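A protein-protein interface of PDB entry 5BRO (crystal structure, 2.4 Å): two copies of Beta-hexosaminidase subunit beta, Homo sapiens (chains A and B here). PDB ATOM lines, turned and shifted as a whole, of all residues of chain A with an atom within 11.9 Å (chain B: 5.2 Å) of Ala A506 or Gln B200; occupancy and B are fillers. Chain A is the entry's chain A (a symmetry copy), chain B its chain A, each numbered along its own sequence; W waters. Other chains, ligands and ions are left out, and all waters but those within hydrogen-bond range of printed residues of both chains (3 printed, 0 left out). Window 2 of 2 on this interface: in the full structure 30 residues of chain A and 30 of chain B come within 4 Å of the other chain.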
ATOM      1  N   TYR A 414      13.542 -26.814 -11.112  1.00  0.00           N
ATOM      2  CA  TYR A 414      13.002 -25.651 -10.451  1.00  0.00           C
ATOM      3  C   TYR A 414      14.091 -24.981  -9.605  1.00  0.00           C
ATOM      4  O   TYR A 414      14.847 -25.661  -8.927  1.00  0.00           O
ATOM      5  CB  TYR A 414      11.849 -26.071  -9.562  1.00  0.00           C
ATOM      6  CG  TYR A 414      11.228 -24.921  -8.839  1.00  0.00           C
ATOM      7  CD1 TYR A 414      10.627 -23.892  -9.540  1.00  0.00           C
ATOM      8  CD2 TYR A 414      11.198 -24.873  -7.448  1.00  0.00           C
ATOM      9  CE1 TYR A 414      10.080 -22.809  -8.890  1.00  0.00           C
ATOM     10  CE2 TYR A 414      10.641 -23.780  -6.785  1.00  0.00           C
ATOM     11  CZ  TYR A 414      10.076 -22.767  -7.528  1.00  0.00           C
ATOM     12  OH  TYR A 414       9.461 -21.731  -6.916  1.00  0.00           O
ATOM     13  N   GLY A 415      14.202 -23.661  -9.675  1.00  0.00           N
ATOM     14  CA  GLY A 415      15.056 -22.926  -8.739  1.00  0.00           C
ATOM     15  C   GLY A 415      16.421 -22.476  -9.254  1.00  0.00           C
ATOM     16  O   GLY A 415      16.707 -22.462 -10.440  1.00  0.00           O
ATOM     17  N   GLN A 416      17.290 -22.100  -8.339  1.00  0.00           N
ATOM     18  CA  GLN A 416      18.566 -21.573  -8.724  1.00  0.00           C
ATOM     19  C   GLN A 416      19.561 -22.656  -9.044  1.00  0.00           C
ATOM     20  O   GLN A 416      20.581 -22.757  -8.392  1.00  0.00           O
ATOM     21  CB  GLN A 416      19.107 -20.689  -7.623  1.00  0.00           C
ATOM     22  CG  GLN A 416      18.116 -19.614  -7.234  1.00  0.00           C
ATOM     23  CD  GLN A 416      18.764 -18.449  -6.524  1.00  0.00           C
ATOM     24  OE1 GLN A 416      19.857 -17.979  -6.900  1.00  0.00           O
ATOM     25  NE2 GLN A 416      18.028 -17.874  -5.580  1.00  0.00           N
ATOM     26  N   TRP A 418      21.696 -22.441 -11.115  1.00  0.00           N
ATOM     27  CA  TRP A 418      22.935 -21.832 -11.605  1.00  0.00           C
ATOM     28  C   TRP A 418      24.065 -22.059 -10.576  1.00  0.00           C
ATOM     29  O   TRP A 418      25.242 -22.177 -10.919  1.00  0.00           O
ATOM     30  CB  TRP A 418      22.729 -20.327 -11.889  1.00  0.00           C
ATOM     31  CG  TRP A 418      22.546 -19.479 -10.671  1.00  0.00           C
ATOM     32  CD1 TRP A 418      21.367 -19.074 -10.125  1.00  0.00           C
ATOM     33  CD2 TRP A 418      23.576 -18.893  -9.875  1.00  0.00           C
ATOM     34  NE1 TRP A 418      21.592 -18.262  -9.039  1.00  0.00           N
ATOM     35  CE2 TRP A 418      22.950 -18.148  -8.861  1.00  0.00           C
ATOM     36  CE3 TRP A 418      24.974 -18.932  -9.918  1.00  0.00           C
ATOM     37  CZ2 TRP A 418      23.672 -17.490  -7.864  1.00  0.00           C
ATOM     38  CZ3 TRP A 418      25.696 -18.235  -8.952  1.00  0.00           C
ATOM     39  CH2 TRP A 418      25.040 -17.576  -7.905  1.00  0.00           C
ATOM     40  N   ARG A 419      23.665 -22.117  -9.318  1.00  0.00           N
ATOM     41  CA  ARG A 419      24.569 -22.414  -8.205  1.00  0.00           C
ATOM     42  C   ARG A 419      25.214 -23.787  -8.345  1.00  0.00           C
ATOM     43  O   ARG A 419      26.416 -23.939  -8.180  1.00  0.00           O
ATOM     44  CB  ARG A 419      23.803 -22.328  -6.893  1.00  0.00           C
ATOM     45  CG  ARG A 419      23.094 -20.997  -6.730  1.00  0.00           C
ATOM     46  CD  ARG A 419      22.459 -20.821  -5.371  1.00  0.00           C
ATOM     47  NE  ARG A 419      21.931 -19.453  -5.290  1.00  0.00           N
ATOM     48  CZ  ARG A 419      22.442 -18.463  -4.545  1.00  0.00           C
ATOM     49  NH1 ARG A 419      23.476 -18.685  -3.713  1.00  0.00           N
ATOM     50  NH2 ARG A 419      21.899 -17.245  -4.617  1.00  0.00           N
ATOM     51  N   PRO A 462      20.910 -16.946 -17.840  1.00  0.00           N
ATOM     52  CA  PRO A 462      22.302 -16.879 -17.414  1.00  0.00           C
ATOM     53  C   PRO A 462      22.856 -18.184 -16.809  1.00  0.00           C
ATOM     54  O   PRO A 462      23.980 -18.212 -16.294  1.00  0.00           O
ATOM     55  CB  PRO A 462      22.277 -15.831 -16.301  1.00  0.00           C
ATOM     56  CG  PRO A 462      20.909 -15.975 -15.745  1.00  0.00           C
ATOM     57  CD  PRO A 462      20.025 -16.186 -16.935  1.00  0.00           C
ATOM     58  N   TYR A 484      26.098 -14.100  -6.775  1.00  0.00           N
ATOM     59  CA  TYR A 484      24.726 -13.755  -7.003  1.00  0.00           C
ATOM     60  C   TYR A 484      24.648 -12.260  -7.361  1.00  0.00           C
ATOM     61  O   TYR A 484      24.024 -11.885  -8.366  1.00  0.00           O
ATOM     62  CB  TYR A 484      23.849 -14.168  -5.803  1.00  0.00           C
ATOM     63  CG  TYR A 484      22.424 -13.660  -5.840  1.00  0.00           C
ATOM     64  CD1 TYR A 484      21.459 -14.279  -6.608  1.00  0.00           C
ATOM     65  CD2 TYR A 484      22.059 -12.537  -5.108  1.00  0.00           C
ATOM     66  CE1 TYR A 484      20.162 -13.823  -6.623  1.00  0.00           C
ATOM     67  CE2 TYR A 484      20.782 -12.029  -5.159  1.00  0.00           C
ATOM     68  CZ  TYR A 484      19.836 -12.675  -5.937  1.00  0.00           C
ATOM     69  OH  TYR A 484      18.566 -12.168  -5.968  1.00  0.00           O
ATOM     70  N   ASP A 485      25.341 -11.424  -6.592  1.00  0.00           N
ATOM     71  CA  ASP A 485      25.286  -9.976  -6.770  1.00  0.00           C
ATOM     72  C   ASP A 485      25.734  -9.608  -8.193  1.00  0.00           C
ATOM     73  O   ASP A 485      25.066  -8.876  -8.871  1.00  0.00           O
ATOM     74  CB  ASP A 485      26.143  -9.270  -5.698  1.00  0.00           C
ATOM     75  CG  ASP A 485      26.197  -7.743  -5.883  1.00  0.00           C
ATOM     76  OD1 ASP A 485      25.215  -7.139  -6.353  1.00  0.00           O
ATOM     77  OD2 ASP A 485      27.224  -7.122  -5.550  1.00  0.00           O
ATOM     78  N   LEU A 487      26.193 -11.621 -10.907  1.00  0.00           N
ATOM     79  CA  LEU A 487      25.394 -12.285 -11.924  1.00  0.00           C
ATOM     80  C   LEU A 487      24.008 -11.665 -12.103  1.00  0.00           C
ATOM     81  O   LEU A 487      23.562 -11.553 -13.234  1.00  0.00           O
ATOM     82  CB  LEU A 487      25.301 -13.788 -11.681  1.00  0.00           C
ATOM     83  CG  LEU A 487      24.837 -14.620 -12.894  1.00  0.00           C
ATOM     84  CD1 LEU A 487      25.713 -14.406 -14.127  1.00  0.00           C
ATOM     85  CD2 LEU A 487      24.753 -16.115 -12.575  1.00  0.00           C
ATOM     86  N   THR A 488      23.375 -11.164 -11.038  1.00  0.00           N
ATOM     87  CA  THR A 488      22.103 -10.459 -11.212  1.00  0.00           C
ATOM     88  C   THR A 488      22.274  -9.240 -12.119  1.00  0.00           C
ATOM     89  O   THR A 488      21.438  -8.981 -12.994  1.00  0.00           O
ATOM     90  CB  THR A 488      21.457  -9.989  -9.888  1.00  0.00           C
ATOM     91  OG1 THR A 488      22.424  -9.327  -9.090  1.00  0.00           O
ATOM     92  CG2 THR A 488      20.962 -11.128  -9.121  1.00  0.00           C
ATOM     93  N   ARG A 489      23.376  -8.517 -11.929  1.00  0.00           N
ATOM     94  CA  ARG A 489      23.645  -7.301 -12.677  1.00  0.00           C
ATOM     95  C   ARG A 489      24.126  -7.592 -14.098  1.00  0.00           C
ATOM     96  O   ARG A 489      23.723  -6.904 -15.024  1.00  0.00           O
ATOM     97  CB  ARG A 489      24.625  -6.436 -11.899  1.00  0.00           C
ATOM     98  CG  ARG A 489      24.019  -6.134 -10.536  1.00  0.00           C
ATOM     99  CD  ARG A 489      24.575  -4.941  -9.820  1.00  0.00           C
ATOM    100  NE  ARG A 489      25.908  -5.165  -9.300  1.00  0.00           N
ATOM    101  CZ  ARG A 489      26.612  -4.176  -8.788  1.00  0.00           C
ATOM    102  NH1 ARG A 489      26.047  -2.976  -8.716  1.00  0.00           N
ATOM    103  NH2 ARG A 489      27.868  -4.363  -8.387  1.00  0.00           N
ATOM    104  N   ARG A 491      23.240 -10.220 -15.750  1.00  0.00           N
ATOM    105  CA  ARG A 491      22.047 -10.673 -16.441  1.00  0.00           C
ATOM    106  C   ARG A 491      21.206  -9.496 -16.839  1.00  0.00           C
ATOM    107  O   ARG A 491      20.754  -9.452 -17.950  1.00  0.00           O
ATOM    108  CB  ARG A 491      21.223 -11.628 -15.584  1.00  0.00           C
ATOM    109  CG  ARG A 491      19.856 -12.004 -16.153  1.00  0.00           C
ATOM    110  CD  ARG A 491      18.739 -11.153 -15.533  1.00  0.00           C
ATOM    111  NE  ARG A 491      17.476 -11.362 -16.234  1.00  0.00           N
ATOM    112  CZ  ARG A 491      16.298 -10.859 -15.879  1.00  0.00           C
ATOM    113  NH1 ARG A 491      16.186 -10.074 -14.824  1.00  0.00           N
ATOM    114  NH2 ARG A 491      15.210 -11.156 -16.591  1.00  0.00           N
ATOM    115  N   CYS A 492      21.051  -8.507 -15.984  1.00  0.00           N
ATOM    116  CA  CYS A 492      20.324  -7.287 -16.388  1.00  0.00           C
ATOM    117  C   CYS A 492      20.945  -6.577 -17.574  1.00  0.00           C
ATOM    118  O   CYS A 492      20.250  -6.105 -18.439  1.00  0.00           O
ATOM    119  CB  CYS A 492      20.234  -6.293 -15.254  1.00  0.00           C
ATOM    120  SG  CYS A 492      18.974  -6.675 -14.032  1.00  0.00           S
ATOM    121  N   ALA A 501      17.942 -13.012 -21.335  1.00  0.00           N
ATOM    122  CA  ALA A 501      18.348 -13.939 -20.281  1.00  0.00           C
ATOM    123  C   ALA A 501      17.412 -13.893 -19.096  1.00  0.00           C
ATOM    124  O   ALA A 501      16.997 -12.829 -18.648  1.00  0.00           O
ATOM    125  CB  ALA A 501      19.769 -13.642 -19.836  1.00  0.00           C
ATOM    126  N   GLN A 502      17.097 -15.049 -18.544  1.00  0.00           N
ATOM    127  CA  GLN A 502      16.060 -15.065 -17.507  1.00  0.00           C
ATOM    128  C   GLN A 502      16.534 -14.665 -16.139  1.00  0.00           C
ATOM    129  O   GLN A 502      17.740 -14.630 -15.873  1.00  0.00           O
ATOM    130  CB  GLN A 502      15.407 -16.424 -17.420  1.00  0.00           C
ATOM    131  CG  GLN A 502      16.286 -17.511 -16.856  1.00  0.00           C
ATOM    132  CD  GLN A 502      15.660 -18.878 -17.022  1.00  0.00           C
ATOM    133  OE1 GLN A 502      14.480 -19.007 -17.374  1.00  0.00           O
ATOM    134  NE2 GLN A 502      16.411 -19.891 -16.698  1.00  0.00           N
ATOM    135  N   PRO A 503      15.583 -14.354 -15.249  1.00  0.00           N
ATOM    136  CA  PRO A 503      15.979 -13.985 -13.915  1.00  0.00           C
ATOM    137  C   PRO A 503      16.650 -15.118 -13.076  1.00  0.00           C
ATOM    138  O   PRO A 503      16.486 -16.318 -13.354  1.00  0.00           O
ATOM    139  CB  PRO A 503      14.670 -13.582 -13.279  1.00  0.00           C
ATOM    140  CG  PRO A 503      13.666 -13.503 -14.378  1.00  0.00           C
ATOM    141  CD  PRO A 503      14.119 -14.473 -15.352  1.00  0.00           C
ATOM    142  N   LEU A 504      17.431 -14.704 -12.078  1.00  0.00           N
ATOM    143  CA  LEU A 504      17.912 -15.606 -11.060  1.00  0.00           C
ATOM    144  C   LEU A 504      16.889 -15.789  -9.987  1.00  0.00           C
ATOM    145  O   LEU A 504      16.806 -16.869  -9.433  1.00  0.00           O
ATOM    146  CB  LEU A 504      19.179 -15.081 -10.388  1.00  0.00           C
ATOM    147  CG  LEU A 504      20.334 -14.679 -11.275  1.00  0.00           C
ATOM    148  CD1 LEU A 504      21.554 -14.610 -10.408  1.00  0.00           C
ATOM    149  CD2 LEU A 504      20.577 -15.661 -12.394  1.00  0.00           C
ATOM    150  N   TYR A 505      16.191 -14.718  -9.618  1.00  0.00           N
ATOM    151  CA  TYR A 505      15.228 -14.764  -8.543  1.00  0.00           C
ATOM    152  C   TYR A 505      14.509 -13.445  -8.616  1.00  0.00           C
ATOM    153  O   TYR A 505      14.751 -12.697  -9.522  1.00  0.00           O
ATOM    154  CB  TYR A 505      15.928 -14.939  -7.163  1.00  0.00           C
ATOM    155  CG  TYR A 505      14.990 -15.278  -6.003  1.00  0.00           C
ATOM    156  CD1 TYR A 505      14.321 -16.474  -5.958  1.00  0.00           C
ATOM    157  CD2 TYR A 505      14.798 -14.395  -4.966  1.00  0.00           C
ATOM    158  CE1 TYR A 505      13.480 -16.787  -4.889  1.00  0.00           C
ATOM    159  CE2 TYR A 505      13.942 -14.681  -3.904  1.00  0.00           C
ATOM    160  CZ  TYR A 505      13.321 -15.892  -3.856  1.00  0.00           C
ATOM    161  OH  TYR A 505      12.442 -16.147  -2.820  1.00  0.00           O
ATOM    162  N   ALA A 506      13.614 -13.176  -7.680  1.00  0.00           N
ATOM    163  CA  ALA A 506      12.865 -11.927  -7.647  1.00  0.00           C
ATOM    164  C   ALA A 506      13.725 -10.701  -7.755  1.00  0.00           C
ATOM    165  O   ALA A 506      14.863 -10.715  -7.354  1.00  0.00           O
ATOM    166  CB  ALA A 506      12.031 -11.851  -6.380  1.00  0.00           C
ATOM    167  N   GLY A 507      13.121  -9.611  -8.204  1.00  0.00           N
ATOM    168  CA  GLY A 507      13.827  -8.365  -8.407  1.00  0.00           C
ATOM    169  C   GLY A 507      13.421  -7.673  -9.694  1.00  0.00           C
ATOM    170  O   GLY A 507      12.384  -7.987 -10.337  1.00  0.00           O
ATOM    171  N   TYR A 508      14.261  -6.726 -10.067  1.00  0.00           N
ATOM    172  CA  TYR A 508      14.000  -5.848 -11.184  1.00  0.00           C
ATOM    173  C   TYR A 508      15.307  -5.367 -11.843  1.00  0.00           C
ATOM    174  O   TYR A 508      16.389  -5.475 -11.270  1.00  0.00           O
ATOM    175  CB  TYR A 508      13.179  -4.675 -10.685  1.00  0.00           C
ATOM    176  CG  TYR A 508      13.956  -3.643  -9.910  1.00  0.00           C
ATOM    177  CD1 TYR A 508      14.371  -3.889  -8.600  1.00  0.00           C
ATOM    178  CD2 TYR A 508      14.192  -2.373 -10.453  1.00  0.00           C
ATOM    179  CE1 TYR A 508      15.010  -2.913  -7.873  1.00  0.00           C
ATOM    180  CE2 TYR A 508      14.833  -1.385  -9.736  1.00  0.00           C
ATOM    181  CZ  TYR A 508      15.230  -1.653  -8.457  1.00  0.00           C
ATOM    182  OH  TYR A 508      15.857  -0.662  -7.765  1.00  0.00           O
ATOM    183  N   CYS A 509      15.217  -4.958 -13.099  1.00  0.00           N
ATOM    184  CA  CYS A 509      16.319  -4.252 -13.748  1.00  0.00           C
ATOM    185  C   CYS A 509      15.941  -2.768 -13.971  1.00  0.00           C
ATOM    186  O   CYS A 509      14.779  -2.508 -14.293  1.00  0.00           O
ATOM    187  CB  CYS A 509      16.617  -4.907 -15.094  1.00  0.00           C
ATOM    188  SG  CYS A 509      17.138  -6.633 -15.038  1.00  0.00           S
ATOM    189  N   ASN A 510      16.848  -1.823 -13.660  1.00  0.00           N
ATOM    190  CA  ASN A 510      17.242  -0.692 -14.591  1.00  0.00           C
ATOM    191  C   ASN A 510      18.075   0.347 -13.870  1.00  0.00           C
ATOM    192  O   ASN A 510      17.939   0.488 -12.656  1.00  0.00           O
ATOM    193  CB  ASN A 510      16.041   0.000 -15.287  1.00  0.00           C
ATOM    194  CG  ASN A 510      16.193   0.070 -16.815  1.00  0.00           C
ATOM    195  OD1 ASN A 510      17.129   0.673 -17.338  1.00  0.00           O
ATOM    196  ND2 ASN A 510      15.262  -0.540 -17.530  1.00  0.00           N
ATOM    197  N   SER B 168       4.569  -9.132  -8.910  1.00  0.00           N
ATOM    198  CA  SER B 168       5.296  -8.555  -7.767  1.00  0.00           C
ATOM    199  C   SER B 168       6.688  -9.092  -7.708  1.00  0.00           C
ATOM    200  O   SER B 168       7.660  -8.366  -7.572  1.00  0.00           O
ATOM    201  CB  SER B 168       4.620  -8.821  -6.437  1.00  0.00           C
ATOM    202  OG  SER B 168       5.356  -8.200  -5.365  1.00  0.00           O
ATOM    203  N   ARG B 169       6.800 -10.390  -7.860  1.00  0.00           N
ATOM    204  CA  ARG B 169       8.098 -10.997  -7.816  1.00  0.00           C
ATOM    205  C   ARG B 169       8.928 -10.467  -8.969  1.00  0.00           C
ATOM    206  O   ARG B 169      10.127 -10.193  -8.786  1.00  0.00           O
ATOM    207  CB  ARG B 169       7.971 -12.515  -7.803  1.00  0.00           C
ATOM    208  CG  ARG B 169       7.678 -13.120  -6.425  1.00  0.00           C
ATOM    209  CD  ARG B 169       6.569 -12.450  -5.653  1.00  0.00           C
ATOM    210  NE  ARG B 169       6.357 -13.129  -4.383  1.00  0.00           N
ATOM    211  CZ  ARG B 169       5.681 -14.280  -4.213  1.00  0.00           C
ATOM    212  NH1 ARG B 169       5.068 -14.900  -5.217  1.00  0.00           N
ATOM    213  NH2 ARG B 169       5.565 -14.803  -3.004  1.00  0.00           N
ATOM    214  N   HIS B 170       8.303 -10.366 -10.151  1.00  0.00           N
ATOM    215  CA  HIS B 170       8.738  -9.437 -11.199  1.00  0.00           C
ATOM    216  C   HIS B 170       7.600  -8.612 -11.720  1.00  0.00           C
ATOM    217  O   HIS B 170       6.449  -9.033 -11.681  1.00  0.00           O
ATOM    218  CB  HIS B 170       9.390 -10.165 -12.351  1.00  0.00           C
ATOM    219  CG  HIS B 170      10.653 -10.861 -11.972  1.00  0.00           C
ATOM    220  ND1 HIS B 170      10.673 -12.142 -11.462  1.00  0.00           N
ATOM    221  CD2 HIS B 170      11.937 -10.433 -11.960  1.00  0.00           C
ATOM    222  CE1 HIS B 170      11.922 -12.489 -11.203  1.00  0.00           C
ATOM    223  NE2 HIS B 170      12.712 -11.485 -11.542  1.00  0.00           N
ATOM    224  N   ASP B 198       2.640  -8.321  -3.619  1.00  0.00           N
ATOM    225  CA  ASP B 198       3.183  -9.344  -2.733  1.00  0.00           C
ATOM    226  C   ASP B 198       4.387  -8.753  -1.976  1.00  0.00           C
ATOM    227  O   ASP B 198       4.528  -7.504  -1.888  1.00  0.00           O
ATOM    228  CB  ASP B 198       3.607 -10.574  -3.526  1.00  0.00           C
ATOM    229  CG  ASP B 198       3.582 -11.867  -2.688  1.00  0.00           C
ATOM    230  OD1 ASP B 198       4.466 -12.016  -1.801  1.00  0.00           O
ATOM    231  OD2 ASP B 198       2.681 -12.719  -2.921  1.00  0.00           O
ATOM    232  N   ASP B 199       5.248  -9.628  -1.445  1.00  0.00           N
ATOM    233  CA  ASP B 199       6.260  -9.196  -0.495  1.00  0.00           C
ATOM    234  C   ASP B 199       7.224  -8.220  -1.165  1.00  0.00           C
ATOM    235  O   ASP B 199       7.488  -7.141  -0.631  1.00  0.00           O
ATOM    236  CB  ASP B 199       7.062 -10.403   0.085  1.00  0.00           C
ATOM    237  CG  ASP B 199       6.372 -11.067   1.267  1.00  0.00           C
ATOM    238  OD1 ASP B 199       5.692 -10.358   2.059  1.00  0.00           O
ATOM    239  OD2 ASP B 199       6.437 -12.318   1.353  1.00  0.00           O
ATOM    240  N   GLN B 200       7.715  -8.609  -2.349  1.00  0.00           N
ATOM    241  CA  GLN B 200       8.865  -7.964  -2.965  1.00  0.00           C
ATOM    242  C   GLN B 200       8.571  -6.555  -3.525  1.00  0.00           C
ATOM    243  O   GLN B 200       9.466  -5.712  -3.578  1.00  0.00           O
ATOM    244  CB  GLN B 200       9.463  -8.844  -4.062  1.00  0.00           C
ATOM    245  CG  GLN B 200      10.154 -10.123  -3.561  1.00  0.00           C
ATOM    246  CD  GLN B 200       9.198 -11.259  -3.234  1.00  0.00           C
ATOM    247  OE1 GLN B 200       7.995 -11.053  -2.987  1.00  0.00           O
ATOM    248  NE2 GLN B 200       9.737 -12.472  -3.209  1.00  0.00           N
ATOM    249  N   SER B 201       7.338  -6.297  -3.941  1.00  0.00           N
ATOM    250  CA  SER B 201       7.005  -5.022  -4.592  1.00  0.00           C
ATOM    251  C   SER B 201       5.501  -4.813  -4.640  1.00  0.00           C
ATOM    252  O   SER B 201       4.730  -5.743  -4.695  1.00  0.00           O
ATOM    253  CB  SER B 201       7.535  -5.020  -6.041  1.00  0.00           C
ATOM    254  OG  SER B 201       6.841  -5.970  -6.844  1.00  0.00           O
ATOM    255  N   PHE B 202       5.091  -3.570  -4.568  1.00  0.00           N
ATOM    256  CA  PHE B 202       3.706  -3.205  -4.739  1.00  0.00           C
ATOM    257  C   PHE B 202       3.571  -2.293  -5.990  1.00  0.00           C
ATOM    258  O   PHE B 202       3.642  -1.074  -5.867  1.00  0.00           O
ATOM    259  CB  PHE B 202       3.283  -2.437  -3.498  1.00  0.00           C
ATOM    260  CG  PHE B 202       1.795  -2.335  -3.302  1.00  0.00           C
ATOM    261  CD1 PHE B 202       1.067  -1.371  -3.962  1.00  0.00           C
ATOM    262  CD2 PHE B 202       1.164  -3.092  -2.330  1.00  0.00           C
ATOM    263  CE1 PHE B 202      -0.304  -1.243  -3.755  1.00  0.00           C
ATOM    264  CE2 PHE B 202      -0.179  -2.914  -2.068  1.00  0.00           C
ATOM    265  CZ  PHE B 202      -0.916  -2.006  -2.793  1.00  0.00           C
ATOM    266  N   GLY B 216       6.487   1.417  -2.353  1.00  0.00           N
ATOM    267  CA  GLY B 216       6.512  -0.042  -2.397  1.00  0.00           C
ATOM    268  C   GLY B 216       6.885  -0.672  -3.727  1.00  0.00           C
ATOM    269  O   GLY B 216       7.192  -1.873  -3.795  1.00  0.00           O
ATOM    270  N   TYR B 218       9.073  -1.423  -7.168  1.00  0.00           N
ATOM    271  CA  TYR B 218      10.489  -1.603  -7.431  1.00  0.00           C
ATOM    272  C   TYR B 218      11.154  -0.258  -7.819  1.00  0.00           C
ATOM    273  O   TYR B 218      12.257   0.012  -7.431  1.00  0.00           O
ATOM    274  CB  TYR B 218      10.664  -2.626  -8.562  1.00  0.00           C
ATOM    275  CG  TYR B 218      10.616  -4.077  -8.152  1.00  0.00           C
ATOM    276  CD1 TYR B 218      11.421  -4.563  -7.109  1.00  0.00           C
ATOM    277  CD2 TYR B 218       9.839  -4.979  -8.854  1.00  0.00           C
ATOM    278  CE1 TYR B 218      11.416  -5.907  -6.780  1.00  0.00           C
ATOM    279  CE2 TYR B 218       9.778  -6.300  -8.487  1.00  0.00           C
ATOM    280  CZ  TYR B 218      10.553  -6.768  -7.455  1.00  0.00           C
ATOM    281  OH  TYR B 218      10.576  -8.123  -7.190  1.00  0.00           O
ATOM    282  N   SER B 255       5.974  -5.480   1.027  1.00  0.00           N
ATOM    283  CA  SER B 255       5.989  -4.251   0.209  1.00  0.00           C
ATOM    284  C   SER B 255       4.923  -3.254   0.613  1.00  0.00           C
ATOM    285  O   SER B 255       5.080  -2.063   0.347  1.00  0.00           O
ATOM    286  CB  SER B 255       5.824  -4.553  -1.286  1.00  0.00           C
ATOM    287  OG  SER B 255       4.460  -4.810  -1.608  1.00  0.00           O
ATOM    288  N   GLU B 449       8.777 -15.640  -8.903  1.00  0.00           N
ATOM    289  CA  GLU B 449      10.139 -15.618  -8.411  1.00  0.00           C
ATOM    290  C   GLU B 449      11.154 -15.833  -9.524  1.00  0.00           C
ATOM    291  O   GLU B 449      12.197 -15.179  -9.517  1.00  0.00           O
ATOM    292  CB  GLU B 449      10.365 -16.717  -7.343  1.00  0.00           C
ATOM    293  CG  GLU B 449       9.715 -16.469  -5.991  1.00  0.00           C
ATOM    294  CD  GLU B 449       8.316 -17.049  -5.905  1.00  0.00           C
ATOM    295  OE1 GLU B 449       7.770 -17.526  -6.956  1.00  0.00           O
ATOM    296  OE2 GLU B 449       7.739 -16.965  -4.797  1.00  0.00           O
HETATM  297  O   HOH W   1      15.217 -10.398 -11.233  1.00  0.00           O
HETATM  298  O   HOH W   2       9.125 -15.425  -2.518  1.00  0.00           O
HETATM  299  O   HOH W   3       8.365 -19.800  -8.341  1.00  0.00           O
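Hydrophobic or aromatic side chains of chain A that line the printed part of chain B: Pro A503, Tyr A505, Ala A506 and Tyr A508.
Of the 12 printed residues of chain B, 5 touch a printed residue of chain A.
Hydrophobic or aromatic side chains of chain B within 4 Å of the printed part of chain A: His B170 and Tyr B218.
Among the printed residues, no Asp or Glu carboxylate lies within 4 Å of a Lys or Arg side-chain nitrogen of the other chain.
N of Gly A507 sits at hydrogen-bond distance from O of Arg B169, at 3.1 Å.
A ring nitrogen (NE2) of His B170 is in hydrogen-bond range of the backbone carbonyl oxygen (O) of Tyr A505, 3.1 Å away.
The side-chain hydroxyl (OH) of Tyr B218 sits at hydrogen-bond distance from the backbone NH (N) of Gly A507, 3.1 Å away.
The backbone NH of Ala A506 lies within hydrogen-bond range of the backbone carbonyl oxygen of Glu B449 (3.1 Å).
His B170 touches Pro A503 (NE2 to CB, 3.4 Å).
Glu B449 touches Tyr A505 (O to C, 3.0 Å).
O of Arg B169 touches CA of Ala A506, 3.4 Å away.
His B170 touches Ala A506 (CE1 to CA, 3.7 Å).
Gln B200 touches Ala A506.
His B170 touches Gly A507.
Tyr B218 touches Tyr A508.
Water W3 lies within hydrogen-bond range of the side-chain hydroxyl of Tyr A414 (2.6 Å) and the side-chain carboxylate of Glu B449 (2.7 Å).
Water W1 bridges NE2 of His B170 (2.7 Å) and O of Tyr A505 (2.9 Å).
Water W2 lies within hydrogen-bond range of the side-chain carboxylate (OE2) of Glu B449 (3.1 Å), the side-chain amide nitrogen (NE2) of Gln B200 (3.1 Å) and the side-chain hydroxyl (OH) of Tyr A505 (3.4 Å).
O of Ser B168 sits at hydrogen-bond distance from OH of Tyr B218, 3.0 Å away.
The guanidinium group (NH2) of Arg B169 is in salt-bridge range of the side-chain carboxylate (OD1) of Asp B198 (3.2 Å).
The guanidinium group (NE) of Arg B169 lies within hydrogen-bond range of the side-chain amide oxygen (OE1) of Gln B200 (3.0 Å).
The side-chain hydroxyl of Tyr B218 is in hydrogen-bond range of the backbone carbonyl oxygen of Arg B169, 2.7 Å away.
NH1 of Arg B169 is in salt-bridge range of OE2 of Glu B449, at 3.4 Å.
The side-chain sulfur (SG) of Cys A509 forms a disulfide with the side-chain sulfur (SG) of Cys A492, at 2.1 Å.
Printed residues of chain B within 4 Å of Pro A503: His B170 (3.4 Å).
Of the printed residues of chain B, Tyr A505 touches His B170 and Glu B449.
Of chain B, only Arg B169, His B170, Gln B200 and Glu B449 come within 4 Å of Ala A506.
Of the printed residues of chain B, Gly A507 touches Arg B169, His B170 and Tyr B218.
Asn A510 touches none of the printed residues of chain B.
No residue of chain A comes within 4 Å of Ser B168.
Arg B169 touches just these residues of chain A: Ala A506 (3.4 Å) and Gly A507 (3.1 Å).
Printed residues of chain A within 4 Å of His B170: Pro A503, Tyr A505, Ala A506 and Gly A507.
No residue of chain A comes within 4 Å of Asp B198.
Gln B200 touches just one residue of chain A: Ala A506 (3.8 Å).
No residue of chain A comes within 4 Å of Ser B201.
Tyr B218 touches just these residues of chain A: Gly A507 and Tyr A508.
Ser B255 touches none of the printed residues of chain A.
Glu B449 touches just these residues of chain A: Tyr A505 (3.0 Å) and Ala A506 (3.1 Å).
The nearest residue of chain A that does not touch Gln B200 is Tyr A505 (4.6 Å).
No position is printed for both chains.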
